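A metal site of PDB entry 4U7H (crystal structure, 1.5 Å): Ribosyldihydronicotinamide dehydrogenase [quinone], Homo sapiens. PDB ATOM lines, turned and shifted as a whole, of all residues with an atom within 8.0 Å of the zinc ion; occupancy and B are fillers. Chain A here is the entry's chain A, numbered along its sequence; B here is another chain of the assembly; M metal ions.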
ATOM      1  N   TYR A 132      22.717 -20.290 -21.986  1.00  0.00           N
ATOM      2  CA  TYR A 132      22.845 -21.475 -21.157  1.00  0.00           C
ATOM      3  C   TYR A 132      23.185 -21.067 -19.718  1.00  0.00           C
ATOM      4  O   TYR A 132      22.379 -20.357 -19.118  1.00  0.00           O
ATOM      5  CB  TYR A 132      23.819 -22.467 -21.777  1.00  0.00           C
ATOM      6  CG  TYR A 132      23.184 -23.129 -23.002  1.00  0.00           C
ATOM      7  CD1 TYR A 132      22.005 -23.853 -22.894  1.00  0.00           C
ATOM      8  CD2 TYR A 132      23.770 -23.008 -24.262  1.00  0.00           C
ATOM      9  CE1 TYR A 132      21.420 -24.455 -24.017  1.00  0.00           C
ATOM     10  CE2 TYR A 132      23.198 -23.603 -25.375  1.00  0.00           C
ATOM     11  CZ  TYR A 132      22.028 -24.328 -25.247  1.00  0.00           C
ATOM     12  OH  TYR A 132      21.474 -24.909 -26.363  1.00  0.00           O
ATOM     13  N   ASP A 133      24.317 -21.469 -19.155  1.00  0.00           N
ATOM     14  CA  ASP A 133      24.533 -21.205 -17.732  1.00  0.00           C
ATOM     15  C   ASP A 133      24.521 -19.703 -17.376  1.00  0.00           C
ATOM     16  O   ASP A 133      24.190 -19.328 -16.237  1.00  0.00           O
ATOM     17  CB  ASP A 133      25.835 -21.829 -17.232  1.00  0.00           C
ATOM     18  CG  ASP A 133      25.729 -23.321 -17.053  1.00  0.00           C
ATOM     19  OD1 ASP A 133      24.624 -23.871 -17.223  1.00  0.00           O
ATOM     20  OD2 ASP A 133      26.754 -23.964 -16.742  1.00  0.00           O
ATOM     21  N   TRP A 169      13.754 -31.983 -24.302  1.00  0.00           N
ATOM     22  CA  TRP A 169      14.960 -31.288 -24.740  1.00  0.00           C
ATOM     23  C   TRP A 169      14.747 -29.885 -25.299  1.00  0.00           C
ATOM     24  O   TRP A 169      15.356 -28.934 -24.805  1.00  0.00           O
ATOM     25  CB  TRP A 169      15.712 -32.187 -25.722  1.00  0.00           C
ATOM     26  CG  TRP A 169      16.938 -31.636 -26.334  1.00  0.00           C
ATOM     27  CD1 TRP A 169      17.120 -31.273 -27.634  1.00  0.00           C
ATOM     28  CD2 TRP A 169      18.211 -31.471 -25.696  1.00  0.00           C
ATOM     29  NE1 TRP A 169      18.403 -30.870 -27.848  1.00  0.00           N
ATOM     30  CE2 TRP A 169      19.108 -30.979 -26.673  1.00  0.00           C
ATOM     31  CE3 TRP A 169      18.672 -31.683 -24.396  1.00  0.00           C
ATOM     32  CZ2 TRP A 169      20.440 -30.691 -26.384  1.00  0.00           C
ATOM     33  CZ3 TRP A 169      19.995 -31.393 -24.117  1.00  0.00           C
ATOM     34  CH2 TRP A 169      20.856 -30.907 -25.104  1.00  0.00           C
ATOM     35  N   LEU A 171      12.374 -27.873 -24.830  1.00  0.00           N
ATOM     36  CA  LEU A 171      11.751 -27.020 -23.804  1.00  0.00           C
ATOM     37  C   LEU A 171      12.687 -26.706 -22.665  1.00  0.00           C
ATOM     38  O   LEU A 171      12.933 -25.539 -22.368  1.00  0.00           O
ATOM     39  CB  LEU A 171      10.498 -27.698 -23.280  1.00  0.00           C
ATOM     40  CG  LEU A 171       9.416 -27.903 -24.354  1.00  0.00           C
ATOM     41  CD1 LEU A 171       8.300 -28.719 -23.767  1.00  0.00           C
ATOM     42  CD2 LEU A 171       8.872 -26.580 -24.897  1.00  0.00           C
ATOM     43  N   GLN A 172      13.213 -27.743 -22.036  1.00  0.00           N
ATOM     44  CA  GLN A 172      14.082 -27.586 -20.878  1.00  0.00           C
ATOM     45  C   GLN A 172      15.441 -27.050 -21.269  1.00  0.00           C
ATOM     46  O   GLN A 172      15.935 -26.076 -20.661  1.00  0.00           O
ATOM     47  CB  GLN A 172      14.256 -28.920 -20.181  1.00  0.00           C
ATOM     48  CG  GLN A 172      12.992 -29.399 -19.523  1.00  0.00           C
ATOM     49  CD  GLN A 172      13.191 -30.535 -18.538  1.00  0.00           C
ATOM     50  OE1 GLN A 172      12.388 -30.710 -17.620  1.00  0.00           O
ATOM     51  NE2 GLN A 172      14.228 -31.355 -18.732  1.00  0.00           N
ATOM     52  N   HIS A 173      16.039 -27.650 -22.285  1.00  0.00           N
ATOM     53  CA  HIS A 173      17.376 -27.230 -22.684  1.00  0.00           C
ATOM     54  C   HIS A 173      17.369 -26.068 -23.679  1.00  0.00           C
ATOM     55  O   HIS A 173      17.945 -25.022 -23.440  1.00  0.00           O
ATOM     56  CB  HIS A 173      18.158 -28.401 -23.265  1.00  0.00           C
ATOM     57  CG  HIS A 173      19.594 -28.084 -23.518  1.00  0.00           C
ATOM     58  ND1 HIS A 173      20.540 -27.970 -22.513  1.00  0.00           N
ATOM     59  CD2 HIS A 173      20.261 -27.838 -24.679  1.00  0.00           C
ATOM     60  CE1 HIS A 173      21.711 -27.670 -23.036  1.00  0.00           C
ATOM     61  NE2 HIS A 173      21.570 -27.589 -24.352  1.00  0.00           N
ATOM     62  N   GLY A 174      16.706 -26.259 -24.824  1.00  0.00           N
ATOM     63  CA  GLY A 174      16.769 -25.268 -25.874  1.00  0.00           C
ATOM     64  C   GLY A 174      16.123 -23.926 -25.537  1.00  0.00           C
ATOM     65  O   GLY A 174      16.450 -22.898 -26.149  1.00  0.00           O
ATOM     66  N   THR A 175      15.174 -23.957 -24.601  1.00  0.00           N
ATOM     67  CA  THR A 175      14.464 -22.751 -24.188  1.00  0.00           C
ATOM     68  C   THR A 175      14.853 -22.335 -22.760  1.00  0.00           C
ATOM     69  O   THR A 175      15.444 -21.296 -22.580  1.00  0.00           O
ATOM     70  CB  THR A 175      12.921 -22.906 -24.337  1.00  0.00           C
ATOM     71  OG1 THR A 175      12.574 -23.388 -25.640  1.00  0.00           O
ATOM     72  CG2 THR A 175      12.194 -21.579 -24.122  1.00  0.00           C
ATOM     73  N   LEU A 176      14.526 -23.146 -21.763  1.00  0.00           N
ATOM     74  CA  LEU A 176      14.648 -22.693 -20.370  1.00  0.00           C
ATOM     75  C   LEU A 176      16.125 -22.582 -19.959  1.00  0.00           C
ATOM     76  O   LEU A 176      16.543 -21.533 -19.522  1.00  0.00           O
ATOM     77  CB  LEU A 176      13.876 -23.581 -19.412  1.00  0.00           C
ATOM     78  CG  LEU A 176      12.366 -23.624 -19.664  1.00  0.00           C
ATOM     79  CD1 LEU A 176      11.740 -24.665 -18.763  1.00  0.00           C
ATOM     80  CD2 LEU A 176      11.717 -22.269 -19.513  1.00  0.00           C
ATOM     81  N   HIS A 177      16.900 -23.646 -20.164  1.00  0.00           N
ATOM     82  CA  HIS A 177      18.332 -23.592 -19.876  1.00  0.00           C
ATOM     83  C   HIS A 177      18.991 -22.483 -20.687  1.00  0.00           C
ATOM     84  O   HIS A 177      19.812 -21.736 -20.167  1.00  0.00           O
ATOM     85  CB  HIS A 177      18.972 -24.933 -20.163  1.00  0.00           C
ATOM     86  CG  HIS A 177      20.391 -25.060 -19.666  1.00  0.00           C
ATOM     87  ND1 HIS A 177      21.101 -26.236 -19.789  1.00  0.00           N
ATOM     88  CD2 HIS A 177      21.202 -24.185 -19.029  1.00  0.00           C
ATOM     89  CE1 HIS A 177      22.306 -26.080 -19.263  1.00  0.00           C
ATOM     90  NE2 HIS A 177      22.390 -24.833 -18.793  1.00  0.00           N
ATOM     91  N   PHE A 178      18.679 -22.402 -21.977  1.00  0.00           N
ATOM     92  CA  PHE A 178      19.259 -21.370 -22.806  1.00  0.00           C
ATOM     93  C   PHE A 178      19.088 -19.994 -22.206  1.00  0.00           C
ATOM     94  O   PHE A 178      19.983 -19.175 -22.269  1.00  0.00           O
ATOM     95  CB  PHE A 178      18.701 -21.416 -24.231  1.00  0.00           C
ATOM     96  CG  PHE A 178      19.420 -20.522 -25.182  1.00  0.00           C
ATOM     97  CD1 PHE A 178      20.617 -20.928 -25.769  1.00  0.00           C
ATOM     98  CD2 PHE A 178      18.919 -19.283 -25.503  1.00  0.00           C
ATOM     99  CE1 PHE A 178      21.280 -20.084 -26.650  1.00  0.00           C
ATOM    100  CE2 PHE A 178      19.564 -18.448 -26.362  1.00  0.00           C
ATOM    101  CZ  PHE A 178      20.765 -18.845 -26.951  1.00  0.00           C
ATOM    102  N   PHE A 181      17.624 -20.241 -16.848  1.00  0.00           N
ATOM    103  CA  PHE A 181      16.910 -20.940 -15.814  1.00  0.00           C
ATOM    104  C   PHE A 181      17.672 -22.185 -15.361  1.00  0.00           C
ATOM    105  O   PHE A 181      18.233 -22.924 -16.177  1.00  0.00           O
ATOM    106  CB  PHE A 181      15.536 -21.411 -16.293  1.00  0.00           C
ATOM    107  CG  PHE A 181      14.508 -20.318 -16.448  1.00  0.00           C
ATOM    108  CD1 PHE A 181      13.788 -19.833 -15.352  1.00  0.00           C
ATOM    109  CD2 PHE A 181      14.209 -19.807 -17.711  1.00  0.00           C
ATOM    110  CE1 PHE A 181      12.805 -18.855 -15.515  1.00  0.00           C
ATOM    111  CE2 PHE A 181      13.227 -18.828 -17.873  1.00  0.00           C
ATOM    112  CZ  PHE A 181      12.524 -18.349 -16.755  1.00  0.00           C
ATOM    113  N   VAL A 183      16.653 -25.688 -14.047  1.00  0.00           N
ATOM    114  CA  VAL A 183      15.456 -26.425 -14.376  1.00  0.00           C
ATOM    115  C   VAL A 183      15.187 -27.447 -13.315  1.00  0.00           C
ATOM    116  O   VAL A 183      15.988 -28.347 -13.103  1.00  0.00           O
ATOM    117  CB  VAL A 183      15.644 -27.112 -15.754  1.00  0.00           C
ATOM    118  CG1 VAL A 183      14.444 -27.978 -16.109  1.00  0.00           C
ATOM    119  CG2 VAL A 183      15.845 -26.063 -16.791  1.00  0.00           C
ATOM    120  N   ILE A 220      17.876 -30.208 -11.974  1.00  0.00           N
ATOM    121  CA  ILE A 220      18.492 -31.284 -12.742  1.00  0.00           C
ATOM    122  C   ILE A 220      19.725 -30.764 -13.439  1.00  0.00           C
ATOM    123  O   ILE A 220      19.853 -29.565 -13.673  1.00  0.00           O
ATOM    124  CB  ILE A 220      17.534 -31.877 -13.796  1.00  0.00           C
ATOM    125  CG1 ILE A 220      17.159 -30.852 -14.877  1.00  0.00           C
ATOM    126  CG2 ILE A 220      16.288 -32.432 -13.133  1.00  0.00           C
ATOM    127  CD1 ILE A 220      16.434 -31.446 -16.097  1.00  0.00           C
ATOM    128  N   PRO A 221      20.668 -31.675 -13.771  1.00  0.00           N
ATOM    129  CA  PRO A 221      21.720 -31.262 -14.688  1.00  0.00           C
ATOM    130  C   PRO A 221      21.131 -31.280 -16.109  1.00  0.00           C
ATOM    131  O   PRO A 221      20.800 -32.353 -16.621  1.00  0.00           O
ATOM    132  CB  PRO A 221      22.801 -32.328 -14.485  1.00  0.00           C
ATOM    133  CG  PRO A 221      22.043 -33.564 -14.090  1.00  0.00           C
ATOM    134  CD  PRO A 221      20.741 -33.104 -13.435  1.00  0.00           C
ATOM    135  N   CYS A 222      20.933 -30.104 -16.684  1.00  0.00           N
ATOM    136  CA  CYS A 222      20.167 -29.999 -17.922  1.00  0.00           C
ATOM    137  C   CYS A 222      21.141 -30.220 -19.051  1.00  0.00           C
ATOM    138  O   CYS A 222      21.587 -29.282 -19.703  1.00  0.00           O
ATOM    139  CB  CYS A 222      19.502 -28.626 -18.030  1.00  0.00           C
ATOM    140  SG  CYS A 222      18.415 -28.517 -19.451  1.00  0.00           S
ATOM    141  N   THR A 223      21.505 -31.483 -19.239  1.00  0.00           N
ATOM    142  CA  THR A 223      22.525 -31.848 -20.217  1.00  0.00           C
ATOM    143  C   THR A 223      21.966 -32.825 -21.214  1.00  0.00           C
ATOM    144  O   THR A 223      20.939 -33.477 -20.974  1.00  0.00           O
ATOM    145  CB  THR A 223      23.691 -32.535 -19.506  1.00  0.00           C
ATOM    146  OG1 THR A 223      23.206 -33.688 -18.833  1.00  0.00           O
ATOM    147  CG2 THR A 223      24.322 -31.618 -18.515  1.00  0.00           C
ATOM    148  N   ALA A 224      22.693 -32.997 -22.320  1.00  0.00           N
ATOM    149  CA  ALA A 224      22.326 -34.011 -23.294  1.00  0.00           C
ATOM    150  C   ALA A 224      22.330 -35.379 -22.626  1.00  0.00           C
ATOM    151  O   ALA A 224      21.440 -36.199 -22.868  1.00  0.00           O
ATOM    152  CB  ALA A 224      23.277 -33.972 -24.486  1.00  0.00           C
ATOM    153  N   TRP A 226      21.647 -36.127 -19.531  1.00  0.00           N
ATOM    154  CA  TRP A 226      20.448 -36.294 -18.729  1.00  0.00           C
ATOM    155  C   TRP A 226      19.264 -36.664 -19.620  1.00  0.00           C
ATOM    156  O   TRP A 226      18.456 -37.532 -19.279  1.00  0.00           O
ATOM    157  CB  TRP A 226      20.129 -35.011 -17.931  1.00  0.00           C
ATOM    158  CG  TRP A 226      18.967 -35.181 -16.985  1.00  0.00           C
ATOM    159  CD1 TRP A 226      19.016 -35.569 -15.673  1.00  0.00           C
ATOM    160  CD2 TRP A 226      17.568 -34.959 -17.275  1.00  0.00           C
ATOM    161  NE1 TRP A 226      17.753 -35.615 -15.131  1.00  0.00           N
ATOM    162  CE2 TRP A 226      16.843 -35.251 -16.097  1.00  0.00           C
ATOM    163  CE3 TRP A 226      16.860 -34.572 -18.424  1.00  0.00           C
ATOM    164  CZ2 TRP A 226      15.458 -35.162 -16.025  1.00  0.00           C
ATOM    165  CZ3 TRP A 226      15.466 -34.478 -18.352  1.00  0.00           C
ATOM    166  CH2 TRP A 226      14.785 -34.768 -17.163  1.00  0.00           C
ATOM    167  N   HIS A 227      19.176 -36.012 -20.771  1.00  0.00           N
ATOM    168  CA  HIS A 227      18.031 -36.207 -21.655  1.00  0.00           C
ATOM    169  C   HIS A 227      18.082 -37.516 -22.465  1.00  0.00           C
ATOM    170  O   HIS A 227      17.055 -38.169 -22.673  1.00  0.00           O
ATOM    171  CB  HIS A 227      17.839 -34.999 -22.603  1.00  0.00           C
ATOM    172  CG  HIS A 227      17.322 -33.761 -21.915  1.00  0.00           C
ATOM    173  ND1 HIS A 227      18.147 -32.880 -21.268  1.00  0.00           N
ATOM    174  CD2 HIS A 227      16.072 -33.268 -21.806  1.00  0.00           C
ATOM    175  CE1 HIS A 227      17.431 -31.890 -20.752  1.00  0.00           C
ATOM    176  NE2 HIS A 227      16.163 -32.104 -21.085  1.00  0.00           N
ATOM    177  N   VAL B 160      27.213 -26.929 -28.124  1.00  0.00           N
ATOM    178  CA  VAL B 160      26.438 -26.517 -26.955  1.00  0.00           C
ATOM    179  C   VAL B 160      24.964 -26.877 -27.102  1.00  0.00           C
ATOM    180  O   VAL B 160      24.271 -27.176 -26.115  1.00  0.00           O
ATOM    181  CB  VAL B 160      26.544 -25.001 -26.690  1.00  0.00           C
ATOM    182  CG1 VAL B 160      27.878 -24.661 -26.044  1.00  0.00           C
ATOM    183  CG2 VAL B 160      26.302 -24.216 -27.974  1.00  0.00           C
HETATM  184 ZN    ZN M   1      20.295 -27.856 -20.575  1.00  0.00          ZN
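O of His 173 sits at hydrogen-bond distance from N of Phe 178. The backbone carbonyl oxygen (O) of Gln 172 is in hydrogen-bond range of the backbone NH (N) of His 177. The backbone carbonyl oxygen of Gln 172 sits close to the side-chain sulfur of Cys 222 (3.7 Å). O of Val 160 of chain B sits at hydrogen-bond distance from NE2 of His 173. A ring nitrogen (NE2) of His 173 sits close to the side-chain hydroxyl (OH) of Tyr 132, 3.4 Å away. A ring nitrogen (NE2) of His 177 lies within hydrogen-bond range of the side-chain carboxylate (OD1) of Asp 133, at 2.9 Å.
ND1 of His 173 is bound to the zinc ion. ND1 of His 177 binds the zinc ion (2.0 Å). The zinc ion is bound by O of Cys 222, 2.1 Å away. SG of Cys 222 is bound to the zinc ion, 2.3 Å away.
Of the 21 residues printed, 3 come within 4 Å of the zinc ion.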
